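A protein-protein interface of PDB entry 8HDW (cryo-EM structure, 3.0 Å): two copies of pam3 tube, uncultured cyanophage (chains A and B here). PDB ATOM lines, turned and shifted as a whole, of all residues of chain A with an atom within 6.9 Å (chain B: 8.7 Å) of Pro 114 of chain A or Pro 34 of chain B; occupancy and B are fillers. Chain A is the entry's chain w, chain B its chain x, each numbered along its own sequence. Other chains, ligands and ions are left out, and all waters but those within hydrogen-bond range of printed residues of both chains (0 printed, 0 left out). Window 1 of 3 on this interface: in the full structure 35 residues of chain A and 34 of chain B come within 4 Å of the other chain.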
ATOM      1  N   HIS A  72      -1.029  -0.228 -26.409  1.00  0.00           N
ATOM      2  CA  HIS A  72      -2.037  -0.918 -25.612  1.00  0.00           C
ATOM      3  C   HIS A  72      -2.146  -2.386 -26.019  1.00  0.00           C
ATOM      4  O   HIS A  72      -2.240  -3.270 -25.161  1.00  0.00           O
ATOM      5  CB  HIS A  72      -3.377  -0.198 -25.757  1.00  0.00           C
ATOM      6  CG  HIS A  72      -4.451  -0.704 -24.846  1.00  0.00           C
ATOM      7  ND1 HIS A  72      -4.309  -0.753 -23.476  1.00  0.00           N
ATOM      8  CD2 HIS A  72      -5.695  -1.167 -25.109  1.00  0.00           C
ATOM      9  CE1 HIS A  72      -5.411  -1.236 -22.938  1.00  0.00           C
ATOM     10  NE2 HIS A  72      -6.268  -1.494 -23.906  1.00  0.00           N
ATOM     11  N   TRP A  79       0.724  -8.951 -20.920  1.00  0.00           N
ATOM     12  CA  TRP A  79      -0.042  -9.348 -19.743  1.00  0.00           C
ATOM     13  C   TRP A  79      -0.513 -10.794 -19.850  1.00  0.00           C
ATOM     14  O   TRP A  79      -0.445 -11.557 -18.881  1.00  0.00           O
ATOM     15  CB  TRP A  79      -1.225  -8.399 -19.577  1.00  0.00           C
ATOM     16  CG  TRP A  79      -2.069  -8.632 -18.375  1.00  0.00           C
ATOM     17  CD1 TRP A  79      -1.687  -9.184 -17.196  1.00  0.00           C
ATOM     18  CD2 TRP A  79      -3.454  -8.315 -18.239  1.00  0.00           C
ATOM     19  NE1 TRP A  79      -2.744  -9.228 -16.329  1.00  0.00           N
ATOM     20  CE2 TRP A  79      -3.844  -8.698 -16.947  1.00  0.00           C
ATOM     21  CE3 TRP A  79      -4.404  -7.740 -19.086  1.00  0.00           C
ATOM     22  CZ2 TRP A  79      -5.140  -8.529 -16.482  1.00  0.00           C
ATOM     23  CZ3 TRP A  79      -5.686  -7.570 -18.620  1.00  0.00           C
ATOM     24  CH2 TRP A  79      -6.044  -7.964 -17.331  1.00  0.00           C
ATOM     25  N   ARG A  83       0.345 -14.081 -17.607  1.00  0.00           N
ATOM     26  CA  ARG A  83      -0.700 -14.895 -16.990  1.00  0.00           C
ATOM     27  C   ARG A  83      -0.564 -16.363 -17.374  1.00  0.00           C
ATOM     28  O   ARG A  83      -0.989 -17.248 -16.625  1.00  0.00           O
ATOM     29  CB  ARG A  83      -2.080 -14.373 -17.383  1.00  0.00           C
ATOM     30  CG  ARG A  83      -2.593 -13.251 -16.517  1.00  0.00           C
ATOM     31  CD  ARG A  83      -3.626 -12.428 -17.250  1.00  0.00           C
ATOM     32  NE  ARG A  83      -4.796 -13.202 -17.632  1.00  0.00           N
ATOM     33  CZ  ARG A  83      -6.023 -12.985 -17.173  1.00  0.00           C
ATOM     34  NH1 ARG A  83      -6.250 -12.008 -16.313  1.00  0.00           N
ATOM     35  NH2 ARG A  83      -7.026 -13.746 -17.585  1.00  0.00           N
ATOM     36  N   LYS A 112       0.295  -3.390 -12.707  1.00  0.00           N
ATOM     37  CA  LYS A 112      -1.127  -3.087 -12.693  1.00  0.00           C
ATOM     38  C   LYS A 112      -1.661  -3.039 -14.116  1.00  0.00           C
ATOM     39  O   LYS A 112      -0.979  -2.614 -15.048  1.00  0.00           O
ATOM     40  CB  LYS A 112      -1.415  -1.753 -11.999  1.00  0.00           C
ATOM     41  CG  LYS A 112      -1.216  -1.741 -10.515  1.00  0.00           C
ATOM     42  CD  LYS A 112      -1.875  -0.514  -9.925  1.00  0.00           C
ATOM     43  CE  LYS A 112      -1.488  -0.296  -8.468  1.00  0.00           C
ATOM     44  NZ  LYS A 112      -0.062   0.097  -8.305  1.00  0.00           N
ATOM     45  N   ALA A 113      -2.910  -3.458 -14.272  1.00  0.00           N
ATOM     46  CA  ALA A 113      -3.592  -3.465 -15.555  1.00  0.00           C
ATOM     47  C   ALA A 113      -4.706  -2.430 -15.524  1.00  0.00           C
ATOM     48  O   ALA A 113      -5.256  -2.146 -14.455  1.00  0.00           O
ATOM     49  CB  ALA A 113      -4.171  -4.849 -15.879  1.00  0.00           C
ATOM     50  N   PRO A 114      -5.044  -1.847 -16.664  1.00  0.00           N
ATOM     51  CA  PRO A 114      -6.014  -0.749 -16.677  1.00  0.00           C
ATOM     52  C   PRO A 114      -7.445  -1.239 -16.522  1.00  0.00           C
ATOM     53  O   PRO A 114      -7.734  -2.434 -16.490  1.00  0.00           O
ATOM     54  CB  PRO A 114      -5.793  -0.115 -18.050  1.00  0.00           C
ATOM     55  CG  PRO A 114      -5.302  -1.205 -18.878  1.00  0.00           C
ATOM     56  CD  PRO A 114      -4.460  -2.061 -17.995  1.00  0.00           C
ATOM     57  N   ASP A 115      -8.350  -0.272 -16.423  1.00  0.00           N
ATOM     58  CA  ASP A 115      -9.784  -0.520 -16.385  1.00  0.00           C
ATOM     59  C   ASP A 115     -10.388  -0.183 -17.740  1.00  0.00           C
ATOM     60  O   ASP A 115     -10.074   0.861 -18.317  1.00  0.00           O
ATOM     61  CB  ASP A 115     -10.450   0.314 -15.295  1.00  0.00           C
ATOM     62  CG  ASP A 115      -9.703   0.263 -13.990  1.00  0.00           C
ATOM     63  OD1 ASP A 115      -8.775  -0.557 -13.870  1.00  0.00           O
ATOM     64  OD2 ASP A 115     -10.035   1.049 -13.084  1.00  0.00           O
ATOM     65  N   ASP A 116     -11.243  -1.065 -18.245  1.00  0.00           N
ATOM     66  CA  ASP A 116     -11.890  -0.867 -19.540  1.00  0.00           C
ATOM     67  C   ASP A 116     -13.228  -0.175 -19.321  1.00  0.00           C
ATOM     68  O   ASP A 116     -14.236  -0.808 -19.019  1.00  0.00           O
ATOM     69  CB  ASP A 116     -12.072  -2.194 -20.261  1.00  0.00           C
ATOM     70  CG  ASP A 116     -10.806  -3.029 -20.276  1.00  0.00           C
ATOM     71  OD1 ASP A 116      -9.721  -2.466 -20.523  1.00  0.00           O
ATOM     72  OD2 ASP A 116     -10.899  -4.252 -20.039  1.00  0.00           O
ATOM     73  N   VAL A 124      -8.861   7.236 -20.353  1.00  0.00           N
ATOM     74  CA  VAL A 124      -7.476   6.787 -20.226  1.00  0.00           C
ATOM     75  C   VAL A 124      -7.395   5.276 -20.032  1.00  0.00           C
ATOM     76  O   VAL A 124      -8.321   4.638 -19.517  1.00  0.00           O
ATOM     77  CB  VAL A 124      -6.814   7.517 -19.044  1.00  0.00           C
ATOM     78  CG1 VAL A 124      -5.304   7.413 -19.102  1.00  0.00           C
ATOM     79  CG2 VAL A 124      -7.256   8.958 -19.006  1.00  0.00           C
ATOM     80  N   ARG A 125      -6.259   4.701 -20.427  1.00  0.00           N
ATOM     81  CA  ARG A 125      -5.855   3.350 -20.055  1.00  0.00           C
ATOM     82  C   ARG A 125      -4.476   3.429 -19.411  1.00  0.00           C
ATOM     83  O   ARG A 125      -3.494   3.722 -20.094  1.00  0.00           O
ATOM     84  CB  ARG A 125      -5.819   2.426 -21.273  1.00  0.00           C
ATOM     85  CG  ARG A 125      -7.109   2.359 -22.055  1.00  0.00           C
ATOM     86  CD  ARG A 125      -8.180   1.588 -21.309  1.00  0.00           C
ATOM     87  NE  ARG A 125      -9.479   2.244 -21.413  1.00  0.00           N
ATOM     88  CZ  ARG A 125     -10.452   1.849 -22.222  1.00  0.00           C
ATOM     89  NH1 ARG A 125     -11.598   2.509 -22.255  1.00  0.00           N
ATOM     90  NH2 ARG A 125     -10.283   0.792 -22.992  1.00  0.00           N
ATOM     91  N   GLU A 126      -4.397   3.160 -18.110  1.00  0.00           N
ATOM     92  CA  GLU A 126      -3.161   3.333 -17.354  1.00  0.00           C
ATOM     93  C   GLU A 126      -2.516   1.992 -17.036  1.00  0.00           C
ATOM     94  O   GLU A 126      -3.128   1.141 -16.387  1.00  0.00           O
ATOM     95  CB  GLU A 126      -3.413   4.082 -16.050  1.00  0.00           C
ATOM     96  CG  GLU A 126      -4.097   5.408 -16.211  1.00  0.00           C
ATOM     97  CD  GLU A 126      -4.253   6.135 -14.896  1.00  0.00           C
ATOM     98  OE1 GLU A 126      -3.587   5.736 -13.917  1.00  0.00           O
ATOM     99  OE2 GLU A 126      -5.042   7.101 -14.841  1.00  0.00           O
ATOM    100  N   TRP A 127      -1.269   1.828 -17.461  1.00  0.00           N
ATOM    101  CA  TRP A 127      -0.471   0.650 -17.169  1.00  0.00           C
ATOM    102  C   TRP A 127       0.626   1.012 -16.178  1.00  0.00           C
ATOM    103  O   TRP A 127       1.063   2.163 -16.119  1.00  0.00           O
ATOM    104  CB  TRP A 127       0.152   0.085 -18.444  1.00  0.00           C
ATOM    105  CG  TRP A 127      -0.824  -0.484 -19.412  1.00  0.00           C
ATOM    106  CD1 TRP A 127      -1.486   0.181 -20.396  1.00  0.00           C
ATOM    107  CD2 TRP A 127      -1.229  -1.849 -19.510  1.00  0.00           C
ATOM    108  NE1 TRP A 127      -2.286  -0.681 -21.093  1.00  0.00           N
ATOM    109  CE2 TRP A 127      -2.144  -1.937 -20.569  1.00  0.00           C
ATOM    110  CE3 TRP A 127      -0.908  -3.008 -18.801  1.00  0.00           C
ATOM    111  CZ2 TRP A 127      -2.743  -3.134 -20.932  1.00  0.00           C
ATOM    112  CZ3 TRP A 127      -1.504  -4.189 -19.166  1.00  0.00           C
ATOM    113  CH2 TRP A 127      -2.411  -4.245 -20.217  1.00  0.00           C
ATOM    114  N   THR A 128       1.064   0.029 -15.400  1.00  0.00           N
ATOM    115  CA  THR A 128       2.144   0.196 -14.433  1.00  0.00           C
ATOM    116  C   THR A 128       3.130  -0.946 -14.617  1.00  0.00           C
ATOM    117  O   THR A 128       2.722  -2.103 -14.741  1.00  0.00           O
ATOM    118  CB  THR A 128       1.607   0.219 -13.002  1.00  0.00           C
ATOM    119  OG1 THR A 128       0.604   1.233 -12.882  1.00  0.00           O
ATOM    120  CG2 THR A 128       2.718   0.503 -12.012  1.00  0.00           C
ATOM    121  N   THR B  31     -17.644  -0.251 -16.757  1.00  0.00           N
ATOM    122  CA  THR B  31     -16.222  -0.265 -16.444  1.00  0.00           C
ATOM    123  C   THR B  31     -15.845  -1.587 -15.796  1.00  0.00           C
ATOM    124  O   THR B  31     -16.506  -2.027 -14.853  1.00  0.00           O
ATOM    125  CB  THR B  31     -15.842   0.905 -15.529  1.00  0.00           C
ATOM    126  OG1 THR B  31     -14.695   0.556 -14.749  1.00  0.00           O
ATOM    127  CG2 THR B  31     -16.983   1.267 -14.617  1.00  0.00           C
ATOM    128  N   THR B  32     -14.785  -2.211 -16.297  1.00  0.00           N
ATOM    129  CA  THR B  32     -14.270  -3.462 -15.758  1.00  0.00           C
ATOM    130  C   THR B  32     -12.896  -3.224 -15.150  1.00  0.00           C
ATOM    131  O   THR B  32     -12.042  -2.590 -15.772  1.00  0.00           O
ATOM    132  CB  THR B  32     -14.168  -4.534 -16.841  1.00  0.00           C
ATOM    133  OG1 THR B  32     -12.943  -4.371 -17.557  1.00  0.00           O
ATOM    134  CG2 THR B  32     -15.309  -4.408 -17.805  1.00  0.00           C
ATOM    135  N   SER B  33     -12.681  -3.740 -13.946  1.00  0.00           N
ATOM    136  CA  SER B  33     -11.391  -3.574 -13.309  1.00  0.00           C
ATOM    137  C   SER B  33     -10.882  -4.907 -12.781  1.00  0.00           C
ATOM    138  O   SER B  33     -11.651  -5.683 -12.207  1.00  0.00           O
ATOM    139  CB  SER B  33     -11.474  -2.565 -12.162  1.00  0.00           C
ATOM    140  OG  SER B  33     -12.346  -3.032 -11.157  1.00  0.00           O
ATOM    141  N   PRO B  34      -9.595  -5.194 -12.955  1.00  0.00           N
ATOM    142  CA  PRO B  34      -9.028  -6.429 -12.411  1.00  0.00           C
ATOM    143  C   PRO B  34      -9.058  -6.452 -10.892  1.00  0.00           C
ATOM    144  O   PRO B  34      -8.998  -5.424 -10.218  1.00  0.00           O
ATOM    145  CB  PRO B  34      -7.590  -6.422 -12.937  1.00  0.00           C
ATOM    146  CG  PRO B  34      -7.313  -5.009 -13.271  1.00  0.00           C
ATOM    147  CD  PRO B  34      -8.607  -4.432 -13.733  1.00  0.00           C
ATOM    148  N   GLY B  35      -9.152  -7.661 -10.357  1.00  0.00           N
ATOM    149  CA  GLY B  35      -9.298  -7.869  -8.932  1.00  0.00           C
ATOM    150  C   GLY B  35      -8.115  -7.479  -8.073  1.00  0.00           C
ATOM    151  O   GLY B  35      -8.303  -6.998  -6.954  1.00  0.00           O
ATOM    152  N   VAL B  36      -6.895  -7.694  -8.560  1.00  0.00           N
ATOM    153  CA  VAL B  36      -5.680  -7.493  -7.783  1.00  0.00           C
ATOM    154  C   VAL B  36      -4.603  -6.892  -8.683  1.00  0.00           C
ATOM    155  O   VAL B  36      -4.806  -6.682  -9.876  1.00  0.00           O
ATOM    156  CB  VAL B  36      -5.179  -8.803  -7.143  1.00  0.00           C
ATOM    157  CG1 VAL B  36      -6.135  -9.278  -6.067  1.00  0.00           C
ATOM    158  CG2 VAL B  36      -5.005  -9.868  -8.201  1.00  0.00           C
ATOM    159  N   ASP B  37      -3.447  -6.611  -8.087  1.00  0.00           N
ATOM    160  CA  ASP B  37      -2.266  -6.237  -8.854  1.00  0.00           C
ATOM    161  C   ASP B  37      -1.667  -7.455  -9.541  1.00  0.00           C
ATOM    162  O   ASP B  37      -1.757  -8.580  -9.051  1.00  0.00           O
ATOM    163  CB  ASP B  37      -1.214  -5.596  -7.954  1.00  0.00           C
ATOM    164  CG  ASP B  37      -1.436  -4.116  -7.756  1.00  0.00           C
ATOM    165  OD1 ASP B  37      -2.494  -3.606  -8.170  1.00  0.00           O
ATOM    166  OD2 ASP B  37      -0.545  -3.455  -7.185  1.00  0.00           O
ATOM    167  N   VAL B  38      -1.035  -7.213 -10.688  1.00  0.00           N
ATOM    168  CA  VAL B  38      -0.465  -8.303 -11.471  1.00  0.00           C
ATOM    169  C   VAL B  38       0.720  -8.929 -10.745  1.00  0.00           C
ATOM    170  O   VAL B  38       0.916 -10.147 -10.792  1.00  0.00           O
ATOM    171  CB  VAL B  38      -0.080  -7.798 -12.874  1.00  0.00           C
ATOM    172  CG1 VAL B  38       0.419  -8.928 -13.734  1.00  0.00           C
ATOM    173  CG2 VAL B  38      -1.255  -7.132 -13.531  1.00  0.00           C
ATOM    174  N   ASP B  56      -4.258 -15.158  -9.935  1.00  0.00           N
ATOM    175  CA  ASP B  56      -5.651 -14.739  -9.799  1.00  0.00           C
ATOM    176  C   ASP B  56      -6.035 -13.915 -11.017  1.00  0.00           C
ATOM    177  O   ASP B  56      -5.484 -12.840 -11.248  1.00  0.00           O
ATOM    178  CB  ASP B  56      -5.837 -13.931  -8.522  1.00  0.00           C
ATOM    179  CG  ASP B  56      -4.783 -14.247  -7.473  1.00  0.00           C
ATOM    180  OD1 ASP B  56      -3.896 -15.084  -7.749  1.00  0.00           O
ATOM    181  OD2 ASP B  56      -4.832 -13.659  -6.370  1.00  0.00           O
ATOM    182  N   LYS B  57      -6.976 -14.419 -11.816  1.00  0.00           N
ATOM    183  CA  LYS B  57      -7.488 -13.674 -12.965  1.00  0.00           C
ATOM    184  C   LYS B  57      -8.990 -13.443 -12.805  1.00  0.00           C
ATOM    185  O   LYS B  57      -9.817 -14.097 -13.431  1.00  0.00           O
ATOM    186  CB  LYS B  57      -7.162 -14.421 -14.249  1.00  0.00           C
ATOM    187  CG  LYS B  57      -7.358 -15.908 -14.165  1.00  0.00           C
ATOM    188  CD  LYS B  57      -6.813 -16.600 -15.387  1.00  0.00           C
ATOM    189  CE  LYS B  57      -5.306 -16.526 -15.430  1.00  0.00           C
ATOM    190  NZ  LYS B  57      -4.742 -17.336 -16.541  1.00  0.00           N
ATOM    191  N   SER B  58      -9.339 -12.436 -12.008  1.00  0.00           N
ATOM    192  CA  SER B  58     -10.728 -12.135 -11.701  1.00  0.00           C
ATOM    193  C   SER B  58     -10.972 -10.645 -11.868  1.00  0.00           C
ATOM    194  O   SER B  58     -10.040  -9.839 -11.852  1.00  0.00           O
ATOM    195  CB  SER B  58     -11.100 -12.564 -10.282  1.00  0.00           C
ATOM    196  OG  SER B  58     -10.306 -11.889  -9.332  1.00  0.00           O
ATOM    197  N   ALA B  59     -12.242 -10.281 -12.027  1.00  0.00           N
ATOM    198  CA  ALA B  59     -12.607  -8.896 -12.274  1.00  0.00           C
ATOM    199  C   ALA B  59     -14.034  -8.637 -11.818  1.00  0.00           C
ATOM    200  O   ALA B  59     -14.831  -9.557 -11.643  1.00  0.00           O
ATOM    201  CB  ALA B  59     -12.462  -8.541 -13.755  1.00  0.00           C
ATOM    202  N   THR B  60     -14.343  -7.356 -11.627  1.00  0.00           N
ATOM    203  CA  THR B  60     -15.702  -6.880 -11.429  1.00  0.00           C
ATOM    204  C   THR B  60     -16.043  -5.926 -12.561  1.00  0.00           C
ATOM    205  O   THR B  60     -15.156  -5.330 -13.169  1.00  0.00           O
ATOM    206  CB  THR B  60     -15.888  -6.144 -10.087  1.00  0.00           C
ATOM    207  OG1 THR B  60     -15.312  -4.838 -10.172  1.00  0.00           O
ATOM    208  CG2 THR B  60     -15.223  -6.886  -8.969  1.00  0.00           C
ATOM    209  N   VAL B  61     -17.333  -5.794 -12.856  1.00  0.00           N
ATOM    210  CA  VAL B  61     -17.805  -4.756 -13.761  1.00  0.00           C
ATOM    211  C   VAL B  61     -18.953  -4.021 -13.089  1.00  0.00           C
ATOM    212  O   VAL B  61     -19.749  -4.621 -12.359  1.00  0.00           O
ATOM    213  CB  VAL B  61     -18.216  -5.300 -15.153  1.00  0.00           C
ATOM    214  CG1 VAL B  61     -17.644  -6.679 -15.402  1.00  0.00           C
ATOM    215  CG2 VAL B  61     -19.709  -5.284 -15.352  1.00  0.00           C
ATOM    216  N   GLU B 101     -11.599  -4.390 -28.786  1.00  0.00           N
ATOM    217  CA  GLU B 101     -11.215  -4.392 -27.383  1.00  0.00           C
ATOM    218  C   GLU B 101     -12.423  -4.722 -26.514  1.00  0.00           C
ATOM    219  O   GLU B 101     -13.527  -4.233 -26.758  1.00  0.00           O
ATOM    220  CB  GLU B 101     -10.631  -3.045 -26.966  1.00  0.00           C
ATOM    221  CG  GLU B 101     -10.170  -3.028 -25.522  1.00  0.00           C
ATOM    222  CD  GLU B 101      -9.887  -1.640 -24.995  1.00  0.00           C
ATOM    223  OE1 GLU B 101      -9.791  -0.697 -25.802  1.00  0.00           O
ATOM    224  OE2 GLU B 101      -9.761  -1.496 -23.763  1.00  0.00           O
ATOM    225  N   THR B 131     -16.765 -11.990 -11.407  1.00  0.00           N
ATOM    226  CA  THR B 131     -16.414 -13.288 -11.960  1.00  0.00           C
ATOM    227  C   THR B 131     -15.081 -13.752 -11.393  1.00  0.00           C
ATOM    228  O   THR B 131     -14.289 -12.961 -10.879  1.00  0.00           O
ATOM    229  CB  THR B 131     -16.342 -13.251 -13.488  1.00  0.00           C
ATOM    230  OG1 THR B 131     -16.185 -14.581 -13.988  1.00  0.00           O
ATOM    231  CG2 THR B 131     -15.182 -12.415 -13.953  1.00  0.00           C
ATOM    232  N   TRP B 134     -11.775 -13.840 -15.988  1.00  0.00           N
ATOM    233  CA  TRP B 134     -12.016 -12.820 -16.999  1.00  0.00           C
ATOM    234  C   TRP B 134     -10.854 -12.841 -17.973  1.00  0.00           C
ATOM    235  O   TRP B 134      -9.700 -12.699 -17.561  1.00  0.00           O
ATOM    236  CB  TRP B 134     -12.163 -11.440 -16.353  1.00  0.00           C
ATOM    237  CG  TRP B 134     -12.165 -10.285 -17.300  1.00  0.00           C
ATOM    238  CD1 TRP B 134     -11.101  -9.523 -17.656  1.00  0.00           C
ATOM    239  CD2 TRP B 134     -13.294  -9.745 -17.991  1.00  0.00           C
ATOM    240  NE1 TRP B 134     -11.487  -8.551 -18.536  1.00  0.00           N
ATOM    241  CE2 TRP B 134     -12.832  -8.665 -18.756  1.00  0.00           C
ATOM    242  CE3 TRP B 134     -14.648 -10.074 -18.042  1.00  0.00           C
ATOM    243  CZ2 TRP B 134     -13.675  -7.909 -19.557  1.00  0.00           C
ATOM    244  CZ3 TRP B 134     -15.480  -9.325 -18.838  1.00  0.00           C
ATOM    245  CH2 TRP B 134     -14.994  -8.258 -19.585  1.00  0.00           C
ATOM    246  N   PRO B 136      -9.405 -10.876 -21.207  1.00  0.00           N
ATOM    247  CA  PRO B 136      -9.514  -9.799 -22.190  1.00  0.00           C
ATOM    248  C   PRO B 136      -9.248 -10.302 -23.596  1.00  0.00           C
ATOM    249  O   PRO B 136      -8.465 -11.224 -23.823  1.00  0.00           O
ATOM    250  CB  PRO B 136      -8.443  -8.800 -21.747  1.00  0.00           C
ATOM    251  CG  PRO B 136      -7.508  -9.585 -20.940  1.00  0.00           C
ATOM    252  CD  PRO B 136      -8.301 -10.649 -20.266  1.00  0.00           C
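NE1 of Trp 127 of chain A lies within hydrogen-bond range of ND1 of His 72 of chain A, 3.1 Å away. The guanidinium group (NE) of Arg 125 of chain A sits at hydrogen-bond distance from the backbone carbonyl oxygen (O) of Asp 115 of chain A (3.4 Å). The backbone NH (N) of Ser 33 of chain B is in hydrogen-bond range of the backbone carbonyl oxygen (O) of Thr 60 of chain B (3.0 Å). The backbone carbonyl oxygen (O) of Lys 57 of chain B is in hydrogen-bond range of the backbone NH (N) of Trp 134 of chain B, 3.2 Å away. The backbone NH (N) of Thr 128 of chain A sits at hydrogen-bond distance from the backbone carbonyl oxygen (O) of Lys 112 of chain A.
OD1 of Asp 116 of chain A sits close to OE2 of Glu 101 of chain B (3.4 Å). NH2 of Arg 125 of chain A is in salt-bridge range of OE2 of Glu 101 of chain B. NE2 of His 72 of chain A sits at hydrogen-bond distance from OE2 of Glu 101 of chain B, at 3.5 Å. The backbone NH (N) of Asp 116 of chain A lies within hydrogen-bond range of the backbone carbonyl oxygen (O) of Thr 32 of chain B (3.0 Å). The side-chain carboxylate (OD2) of Asp 37 of chain B is in salt-bridge range of the side-chain amino group (NZ) of Lys 112 of chain A, 3.8 Å away. The guanidinium group of Arg 83 of chain A is in hydrogen-bond range of the backbone carbonyl oxygen of Trp 134 of chain B (2.9 Å).
Of the printed residues of chain B, Trp 79 of chain A touches Val 38 and Pro 136. Printed residues of chain B within 4 Å of Lys 112 of chain A: Asp 37. Of chain B, only Pro 34 comes within 4 Å of Ala 113 of chain A. Of chain B, only Pro 34 comes within 4 Å of Pro 114 of chain A. Of the printed residues of chain B, Asp 115 of chain A touches Thr 32, Ser 33 and Pro 34. Printed residues of chain A within 4 Å of Lys 57 of chain B: Arg 83. The nearest residue of chain B that does not touch Pro 114 of chain A is Thr 32 of chain B (4.4 Å). The nearest residue of chain A that does not touch Pro 34 of chain B is Trp 79 of chain A (4.8 Å).
NE1 of Trp 79 of chain A touches CG2 of Val 38 of chain B (3.8 Å). Trp 79 of chain A touches Pro 136 of chain B (CZ3 to CG, 3.6 Å). CB of Lys 57 of chain B touches NH1 of Arg 83 of chain A, 3.3 Å away. Pro 34 of chain B touches Ala 113 of chain A (CG to O, 3.7 Å). Pro 34 of chain B touches Pro 114 of chain A (CD to O, 3.5 Å). Thr 32 of chain B touches Asp 115 of chain A (O to CA, 3.1 Å). Ser 33 of chain B touches Asp 115 of chain A. Pro 34 of chain B touches Asp 115 of chain A. Thr 31 of chain B touches Asp 116 of chain A (CA to O, 3.3 Å).
Of the 13 printed residues of chain A, 9 touch a printed residue of chain B. Printed residues of chain A that touch a printed residue of chain B: His 72, Trp 79, Arg 83, Lys 112, Ala 113, Pro 114, Asp 115, Asp 116 and Arg 125. Hydrophobic or aromatic side chains of chain A that line the printed part of chain B: His 72 and Trp 79. Along chain A the printed residues that touch a printed residue of chain B span positions 72 to 125. Of the 18 printed residues of chain B, 10 touch a printed residue of chain A. Printed residues of chain B that touch a printed residue of chain A: Thr 31, Thr 32, Ser 33, Pro 34, Asp 37, Val 38, Lys 57, Glu 101, Trp 134 and Pro 136.
No position is printed for both chains.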
